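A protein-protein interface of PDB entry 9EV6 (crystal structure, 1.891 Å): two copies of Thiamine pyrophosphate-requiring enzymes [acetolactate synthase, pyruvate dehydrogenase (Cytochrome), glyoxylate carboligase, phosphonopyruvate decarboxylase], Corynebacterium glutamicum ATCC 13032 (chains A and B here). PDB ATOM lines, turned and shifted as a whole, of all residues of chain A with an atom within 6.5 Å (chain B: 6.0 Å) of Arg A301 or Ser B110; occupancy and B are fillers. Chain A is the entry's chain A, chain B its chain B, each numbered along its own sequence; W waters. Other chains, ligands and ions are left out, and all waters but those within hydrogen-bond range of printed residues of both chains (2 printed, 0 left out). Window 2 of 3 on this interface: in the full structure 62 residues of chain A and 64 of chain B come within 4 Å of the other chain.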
ATOM      1  N   ARG A  91      11.455  -6.280 -11.159  1.00  0.00           N
ATOM      2  CA  ARG A  91      11.158  -5.291 -10.117  1.00  0.00           C
ATOM      3  C   ARG A  91      12.143  -5.400  -8.950  1.00  0.00           C
ATOM      4  O   ARG A  91      12.485  -4.384  -8.345  1.00  0.00           O
ATOM      5  CB  ARG A  91       9.726  -5.442  -9.586  1.00  0.00           C
ATOM      6  CG  ARG A  91       8.600  -5.169 -10.588  1.00  0.00           C
ATOM      7  CD  ARG A  91       8.542  -3.738 -11.083  1.00  0.00           C
ATOM      8  NE  ARG A  91       8.518  -2.737 -10.011  1.00  0.00           N
ATOM      9  CZ  ARG A  91       7.417  -2.230  -9.463  1.00  0.00           C
ATOM     10  NH1 ARG A  91       6.223  -2.614  -9.877  1.00  0.00           N
ATOM     11  NH2 ARG A  91       7.508  -1.315  -8.512  1.00  0.00           N
ATOM     12  N   ASP A 277      11.889   3.780  -2.634  1.00  0.00           N
ATOM     13  CA  ASP A 277      10.868   4.123  -3.613  1.00  0.00           C
ATOM     14  C   ASP A 277       9.484   3.710  -3.064  1.00  0.00           C
ATOM     15  O   ASP A 277       8.609   3.334  -3.830  1.00  0.00           O
ATOM     16  CB  ASP A 277      11.174   3.512  -4.991  1.00  0.00           C
ATOM     17  CG  ASP A 277      10.326   4.079  -6.123  1.00  0.00           C
ATOM     18  OD1 ASP A 277       9.993   5.299  -6.078  1.00  0.00           O
ATOM     19  OD2 ASP A 277       9.946   3.302  -7.017  1.00  0.00           O
ATOM     20  N   PRO A 279       5.935   3.427  -2.197  1.00  0.00           N
ATOM     21  CA  PRO A 279       4.944   4.030  -3.105  1.00  0.00           C
ATOM     22  C   PRO A 279       3.692   4.642  -2.494  1.00  0.00           C
ATOM     23  O   PRO A 279       2.921   5.255  -3.229  1.00  0.00           O
ATOM     24  CB  PRO A 279       4.523   2.848  -3.985  1.00  0.00           C
ATOM     25  CG  PRO A 279       4.711   1.660  -3.126  1.00  0.00           C
ATOM     26  CD  PRO A 279       5.889   1.955  -2.235  1.00  0.00           C
ATOM     27  N   SER A 281       2.079   7.291  -1.146  1.00  0.00           N
ATOM     28  CA  SER A 281       2.115   8.747  -1.032  1.00  0.00           C
ATOM     29  C   SER A 281       1.273   9.321   0.098  1.00  0.00           C
ATOM     30  O   SER A 281       1.689  10.312   0.689  1.00  0.00           O
ATOM     31  CB  SER A 281       1.641   9.374  -2.332  1.00  0.00           C
ATOM     32  OG  SER A 281       2.426   8.881  -3.403  1.00  0.00           O
ATOM     33  N   GLN A 291      15.562  13.714  -0.955  1.00  0.00           N
ATOM     34  CA  GLN A 291      15.610  12.345  -1.424  1.00  0.00           C
ATOM     35  C   GLN A 291      16.937  12.066  -2.051  1.00  0.00           C
ATOM     36  O   GLN A 291      17.347  12.792  -2.948  1.00  0.00           O
ATOM     37  CB  GLN A 291      14.461  12.003  -2.403  1.00  0.00           C
ATOM     38  CG  GLN A 291      14.527  10.549  -2.860  1.00  0.00           C
ATOM     39  CD  GLN A 291      13.257  10.056  -3.493  1.00  0.00           C
ATOM     40  OE1 GLN A 291      12.411  10.836  -3.963  1.00  0.00           O
ATOM     41  NE2 GLN A 291      13.090   8.738  -3.513  1.00  0.00           N
ATOM     42  N   ASN A 295      19.336   6.402  -8.943  1.00  0.00           N
ATOM     43  CA  ASN A 295      18.703   6.569 -10.229  1.00  0.00           C
ATOM     44  C   ASN A 295      17.907   7.883 -10.168  1.00  0.00           C
ATOM     45  O   ASN A 295      16.861   7.942  -9.527  1.00  0.00           O
ATOM     46  CB  ASN A 295      17.815   5.348 -10.564  1.00  0.00           C
ATOM     47  CG  ASN A 295      17.234   5.433 -11.978  1.00  0.00           C
ATOM     48  OD1 ASN A 295      17.106   6.519 -12.563  1.00  0.00           O
ATOM     49  ND2 ASN A 295      16.883   4.297 -12.578  1.00  0.00           N
ATOM     50  N   ALA A 297      15.940   9.299 -12.168  1.00  0.00           N
ATOM     51  CA  ALA A 297      14.555   9.225 -12.653  1.00  0.00           C
ATOM     52  C   ALA A 297      13.554   8.841 -11.533  1.00  0.00           C
ATOM     53  O   ALA A 297      12.352   9.102 -11.679  1.00  0.00           O
ATOM     54  CB  ALA A 297      14.447   8.225 -13.796  1.00  0.00           C
ATOM     55  N   HIS A 298      14.035   8.225 -10.438  1.00  0.00           N
ATOM     56  CA  HIS A 298      13.161   7.805  -9.337  1.00  0.00           C
ATOM     57  C   HIS A 298      12.872   8.923  -8.346  1.00  0.00           C
ATOM     58  O   HIS A 298      12.016   8.735  -7.485  1.00  0.00           O
ATOM     59  CB  HIS A 298      13.784   6.634  -8.547  1.00  0.00           C
ATOM     60  CG  HIS A 298      13.956   5.356  -9.318  1.00  0.00           C
ATOM     61  ND1 HIS A 298      14.350   4.183  -8.689  1.00  0.00           N
ATOM     62  CD2 HIS A 298      13.798   5.103 -10.637  1.00  0.00           C
ATOM     63  CE1 HIS A 298      14.435   3.278  -9.643  1.00  0.00           C
ATOM     64  NE2 HIS A 298      14.130   3.788 -10.827  1.00  0.00           N
ATOM     65  N   ILE A 299      13.644  10.022  -8.361  1.00  0.00           N
ATOM     66  CA  ILE A 299      13.475  11.070  -7.361  1.00  0.00           C
ATOM     67  C   ILE A 299      12.149  11.809  -7.562  1.00  0.00           C
ATOM     68  O   ILE A 299      11.788  12.136  -8.696  1.00  0.00           O
ATOM     69  CB  ILE A 299      14.673  12.023  -7.392  1.00  0.00           C
ATOM     70  CG1 ILE A 299      15.968  11.259  -7.073  1.00  0.00           C
ATOM     71  CG2 ILE A 299      14.464  13.209  -6.447  1.00  0.00           C
ATOM     72  CD1 ILE A 299      17.237  12.108  -7.263  1.00  0.00           C
ATOM     73  N   GLY A 300      11.428  12.035  -6.461  1.00  0.00           N
ATOM     74  CA  GLY A 300      10.165  12.765  -6.492  1.00  0.00           C
ATOM     75  C   GLY A 300       8.991  11.999  -7.050  1.00  0.00           C
ATOM     76  O   GLY A 300       7.938  12.581  -7.303  1.00  0.00           O
ATOM     77  N   ARG A 301       9.133  10.702  -7.220  1.00  0.00           N
ATOM     78  CA  ARG A 301       8.052   9.860  -7.712  1.00  0.00           C
ATOM     79  C   ARG A 301       6.885   9.774  -6.729  1.00  0.00           C
ATOM     80  O   ARG A 301       5.744   9.555  -7.144  1.00  0.00           O
ATOM     81  CB  ARG A 301       8.610   8.444  -7.865  1.00  0.00           C
ATOM     82  CG  ARG A 301       8.532   7.851  -9.241  1.00  0.00           C
ATOM     83  CD  ARG A 301       9.096   6.436  -9.180  1.00  0.00           C
ATOM     84  NE  ARG A 301       9.703   6.074 -10.453  1.00  0.00           N
ATOM     85  CZ  ARG A 301      10.380   4.957 -10.678  1.00  0.00           C
ATOM     86  NH1 ARG A 301      10.536   4.059  -9.713  1.00  0.00           N
ATOM     87  NH2 ARG A 301      10.913   4.728 -11.872  1.00  0.00           N
ATOM     88  N   ARG A 302       7.174   9.885  -5.407  1.00  0.00           N
ATOM     89  CA  ARG A 302       6.176   9.568  -4.381  1.00  0.00           C
ATOM     90  C   ARG A 302       5.627  10.751  -3.580  1.00  0.00           C
ATOM     91  O   ARG A 302       4.545  10.638  -3.012  1.00  0.00           O
ATOM     92  CB  ARG A 302       6.771   8.529  -3.413  1.00  0.00           C
ATOM     93  CG  ARG A 302       7.415   7.338  -4.145  1.00  0.00           C
ATOM     94  CD  ARG A 302       6.395   6.567  -4.993  1.00  0.00           C
ATOM     95  NE  ARG A 302       7.042   5.449  -5.676  1.00  0.00           N
ATOM     96  CZ  ARG A 302       6.488   4.743  -6.657  1.00  0.00           C
ATOM     97  NH1 ARG A 302       5.260   5.035  -7.088  1.00  0.00           N
ATOM     98  NH2 ARG A 302       7.159   3.754  -7.225  1.00  0.00           N
ATOM     99  N   THR A 303       6.343  11.860  -3.514  1.00  0.00           N
ATOM    100  CA  THR A 303       5.880  13.054  -2.794  1.00  0.00           C
ATOM    101  C   THR A 303       6.664  14.276  -3.293  1.00  0.00           C
ATOM    102  O   THR A 303       7.540  14.139  -4.144  1.00  0.00           O
ATOM    103  CB  THR A 303       5.997  12.851  -1.258  1.00  0.00           C
ATOM    104  OG1 THR A 303       5.239  13.875  -0.599  1.00  0.00           O
ATOM    105  CG2 THR A 303       7.446  12.850  -0.762  1.00  0.00           C
ATOM    106  N   VAL A 305       9.508  16.653  -3.442  1.00  0.00           N
ATOM    107  CA  VAL A 305      10.891  16.617  -3.013  1.00  0.00           C
ATOM    108  C   VAL A 305      11.500  17.987  -3.298  1.00  0.00           C
ATOM    109  O   VAL A 305      11.513  18.417  -4.447  1.00  0.00           O
ATOM    110  CB  VAL A 305      11.687  15.476  -3.690  1.00  0.00           C
ATOM    111  CG1 VAL A 305      13.186  15.618  -3.408  1.00  0.00           C
ATOM    112  CG2 VAL A 305      11.178  14.110  -3.216  1.00  0.00           C
ATOM    113  N   ALA B 106      -4.966   6.844 -10.537  1.00  0.00           N
ATOM    114  CA  ALA B 106      -4.059   7.920 -10.088  1.00  0.00           C
ATOM    115  C   ALA B 106      -2.591   7.457 -10.013  1.00  0.00           C
ATOM    116  O   ALA B 106      -1.700   8.302  -9.999  1.00  0.00           O
ATOM    117  CB  ALA B 106      -4.498   8.436  -8.717  1.00  0.00           C
ATOM    118  N   GLN B 107      -2.344   6.138  -9.943  1.00  0.00           N
ATOM    119  CA  GLN B 107      -0.989   5.594  -9.825  1.00  0.00           C
ATOM    120  C   GLN B 107      -0.406   5.112 -11.155  1.00  0.00           C
ATOM    121  O   GLN B 107       0.765   4.708 -11.191  1.00  0.00           O
ATOM    122  CB  GLN B 107      -0.977   4.426  -8.822  1.00  0.00           C
ATOM    123  CG  GLN B 107      -1.401   4.830  -7.413  1.00  0.00           C
ATOM    124  CD  GLN B 107      -0.425   5.828  -6.812  1.00  0.00           C
ATOM    125  OE1 GLN B 107       0.762   5.892  -7.159  1.00  0.00           O
ATOM    126  NE2 GLN B 107      -0.903   6.646  -5.894  1.00  0.00           N
ATOM    127  N   ILE B 108      -1.193   5.131 -12.252  1.00  0.00           N
ATOM    128  CA  ILE B 108      -0.665   4.681 -13.554  1.00  0.00           C
ATOM    129  C   ILE B 108       0.480   5.605 -13.987  1.00  0.00           C
ATOM    130  O   ILE B 108       0.361   6.829 -13.895  1.00  0.00           O
ATOM    131  CB  ILE B 108      -1.788   4.601 -14.610  1.00  0.00           C
ATOM    132  CG1 ILE B 108      -2.752   3.442 -14.258  1.00  0.00           C
ATOM    133  CG2 ILE B 108      -1.202   4.436 -16.030  1.00  0.00           C
ATOM    134  CD1 ILE B 108      -4.042   3.397 -15.139  1.00  0.00           C
ATOM    135  N   GLY B 109       1.605   5.017 -14.351  1.00  0.00           N
ATOM    136  CA  GLY B 109       2.766   5.784 -14.774  1.00  0.00           C
ATOM    137  C   GLY B 109       3.739   6.128 -13.664  1.00  0.00           C
ATOM    138  O   GLY B 109       4.765   6.778 -13.908  1.00  0.00           O
ATOM    139  N   SER B 110       3.440   5.701 -12.427  1.00  0.00           N
ATOM    140  CA  SER B 110       4.315   5.985 -11.296  1.00  0.00           C
ATOM    141  C   SER B 110       5.116   4.771 -10.873  1.00  0.00           C
ATOM    142  O   SER B 110       5.660   4.801  -9.786  1.00  0.00           O
ATOM    143  CB  SER B 110       3.489   6.479 -10.108  1.00  0.00           C
ATOM    144  OG  SER B 110       2.995   7.780 -10.388  1.00  0.00           O
ATOM    145  N   THR B 111       5.198   3.668 -11.685  1.00  0.00           N
ATOM    146  CA  THR B 111       5.917   2.428 -11.283  1.00  0.00           C
ATOM    147  C   THR B 111       5.408   1.988  -9.900  1.00  0.00           C
ATOM    148  O   THR B 111       6.168   1.829  -8.933  1.00  0.00           O
ATOM    149  CB  THR B 111       7.469   2.593 -11.316  1.00  0.00           C
ATOM    150  OG1 THR B 111       7.833   3.246 -12.528  1.00  0.00           O
ATOM    151  CG2 THR B 111       8.197   1.242 -11.237  1.00  0.00           C
ATOM    152  N   PHE B 112       4.079   1.954  -9.787  1.00  0.00           N
ATOM    153  CA  PHE B 112       3.445   1.663  -8.503  1.00  0.00           C
ATOM    154  C   PHE B 112       3.591   0.200  -8.168  1.00  0.00           C
ATOM    155  O   PHE B 112       3.963  -0.621  -9.014  1.00  0.00           O
ATOM    156  CB  PHE B 112       1.938   2.053  -8.594  1.00  0.00           C
ATOM    157  CG  PHE B 112       1.188   2.025  -7.284  1.00  0.00           C
ATOM    158  CD1 PHE B 112       1.569   2.844  -6.232  1.00  0.00           C
ATOM    159  CD2 PHE B 112       0.069   1.224  -7.123  1.00  0.00           C
ATOM    160  CE1 PHE B 112       0.871   2.834  -5.030  1.00  0.00           C
ATOM    161  CE2 PHE B 112      -0.616   1.194  -5.910  1.00  0.00           C
ATOM    162  CZ  PHE B 112      -0.219   2.011  -4.875  1.00  0.00           C
ATOM    163  N   GLU B 115       2.290  -2.571 -10.587  1.00  0.00           N
ATOM    164  CA  GLU B 115       2.030  -2.000 -11.922  1.00  0.00           C
ATOM    165  C   GLU B 115       2.581  -2.846 -13.081  1.00  0.00           C
ATOM    166  O   GLU B 115       3.747  -3.258 -13.090  1.00  0.00           O
ATOM    167  CB  GLU B 115       2.598  -0.578 -12.070  1.00  0.00           C
ATOM    168  CG  GLU B 115       2.205   0.083 -13.393  1.00  0.00           C
ATOM    169  CD  GLU B 115       2.320   1.599 -13.431  1.00  0.00           C
ATOM    170  OE1 GLU B 115       2.730   2.189 -12.402  1.00  0.00           O
ATOM    171  OE2 GLU B 115       1.982   2.200 -14.485  1.00  0.00           O
HETATM  172  O   HOH W   1       5.166  -4.776 -11.273  1.00  0.00           O
HETATM  173  O   HOH W   2       3.145   6.506  -5.870  1.00  0.00           O
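Water W1 lies within hydrogen-bond range of the backbone carbonyl oxygen (O) of Glu B115 (2.8 Å) and the guanidinium group (NH1) of Arg A91 (2.8 Å). Water W2 lies within hydrogen-bond range of the side-chain amide oxygen (OE1) of Gln B107 (2.8 Å), the guanidinium group (NH1) of Arg A302 (2.8 Å), the backbone carbonyl oxygen (O) of Pro A279 (2.9 Å) and the side-chain hydroxyl (OG) of Ser A281 (3.5 Å).
The guanidinium group (NH2) of Arg A302 is in hydrogen-bond range of the backbone carbonyl oxygen (O) of Thr B111 (2.8 Å). The guanidinium group of Arg A91 is in hydrogen-bond range of the backbone carbonyl oxygen of Thr B111. NH1 of Arg A91 is in hydrogen-bond range of O of Phe B112, at 3.1 Å. The guanidinium group (NH2) of Arg A301 sits at hydrogen-bond distance from the side-chain hydroxyl (OG1) of Thr B111 (3.5 Å). O of Ser B110 lies within hydrogen-bond range of NH1 of Arg A302 (2.7 Å).
Arg A91 touches Glu B115 (NH1 to N, 3.997 Å). O of Pro A279 touches CE1 of Phe B112 (3.6 Å). Arg A301 touches Ser B110.
The backbone NH of Thr B111 sits at hydrogen-bond distance from the side-chain carboxylate of Glu B115 (3.0 Å). The guanidinium group (NH2) of Arg A302 is in salt-bridge range of the side-chain carboxylate (OD2) of Asp A277, at 2.8 Å. N of Phe B112 is in hydrogen-bond range of OE1 of Glu B115 (3.0 Å). The side-chain carboxylate of Asp A277 is in salt-bridge range of the guanidinium group of Arg A301, at 2.9 Å. The backbone NH of Gly B109 sits at hydrogen-bond distance from the side-chain carboxylate of Glu B115 (2.8 Å). OG of Ser A281 lies within hydrogen-bond range of O of Arg A302, at 2.8 Å.
No position is printed for both chains. Of the 8 pairs that touch across the chains among the printed residues, none has its exchanged pair printed and touching as well.
Printed residues of chain A that touch a printed residue of chain B: Arg A91, Pro A279, Arg A301 and Arg A302. Hydrophobic or aromatic side chains of chain B within 4 Å of the printed part of chain A: Phe B112. Among the printed residues, 8 pairs touch across the chains. Among the printed residues, no Asp or Glu carboxylate lies within 4 Å of a Lys or Arg side-chain nitrogen of the other chain.
Printed residues of chain B within 4 Å of Pro A279: Phe B112. Ile A299 touches none of the printed residues of chain B. Arg A301 touches two residues of chain B. Gly B109 touches none of the printed residues of chain A. Printed residues of chain A within 4 Å of Ser B110: Arg A301 (3.9 Å) and Arg A302 (2.7 Å). Of the printed residues of chain A, Thr B111 touches Arg A91 (3.4 Å), Arg A301 (3.5 Å) and Arg A302 (2.8 Å). Printed residues of chain A within 4 Å of Phe B112: Arg A91 (3.1 Å) and Pro A279 (3.6 Å). Of the printed residues of chain A, Glu B115 touches Arg A91 (3.997 Å). The nearest residue of chain A that does not touch Ser B110 is Asp A277 (5.3 Å). The nearest printed residue of chain B that does not touch Arg A91 is Ser B110 (6.5 Å).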
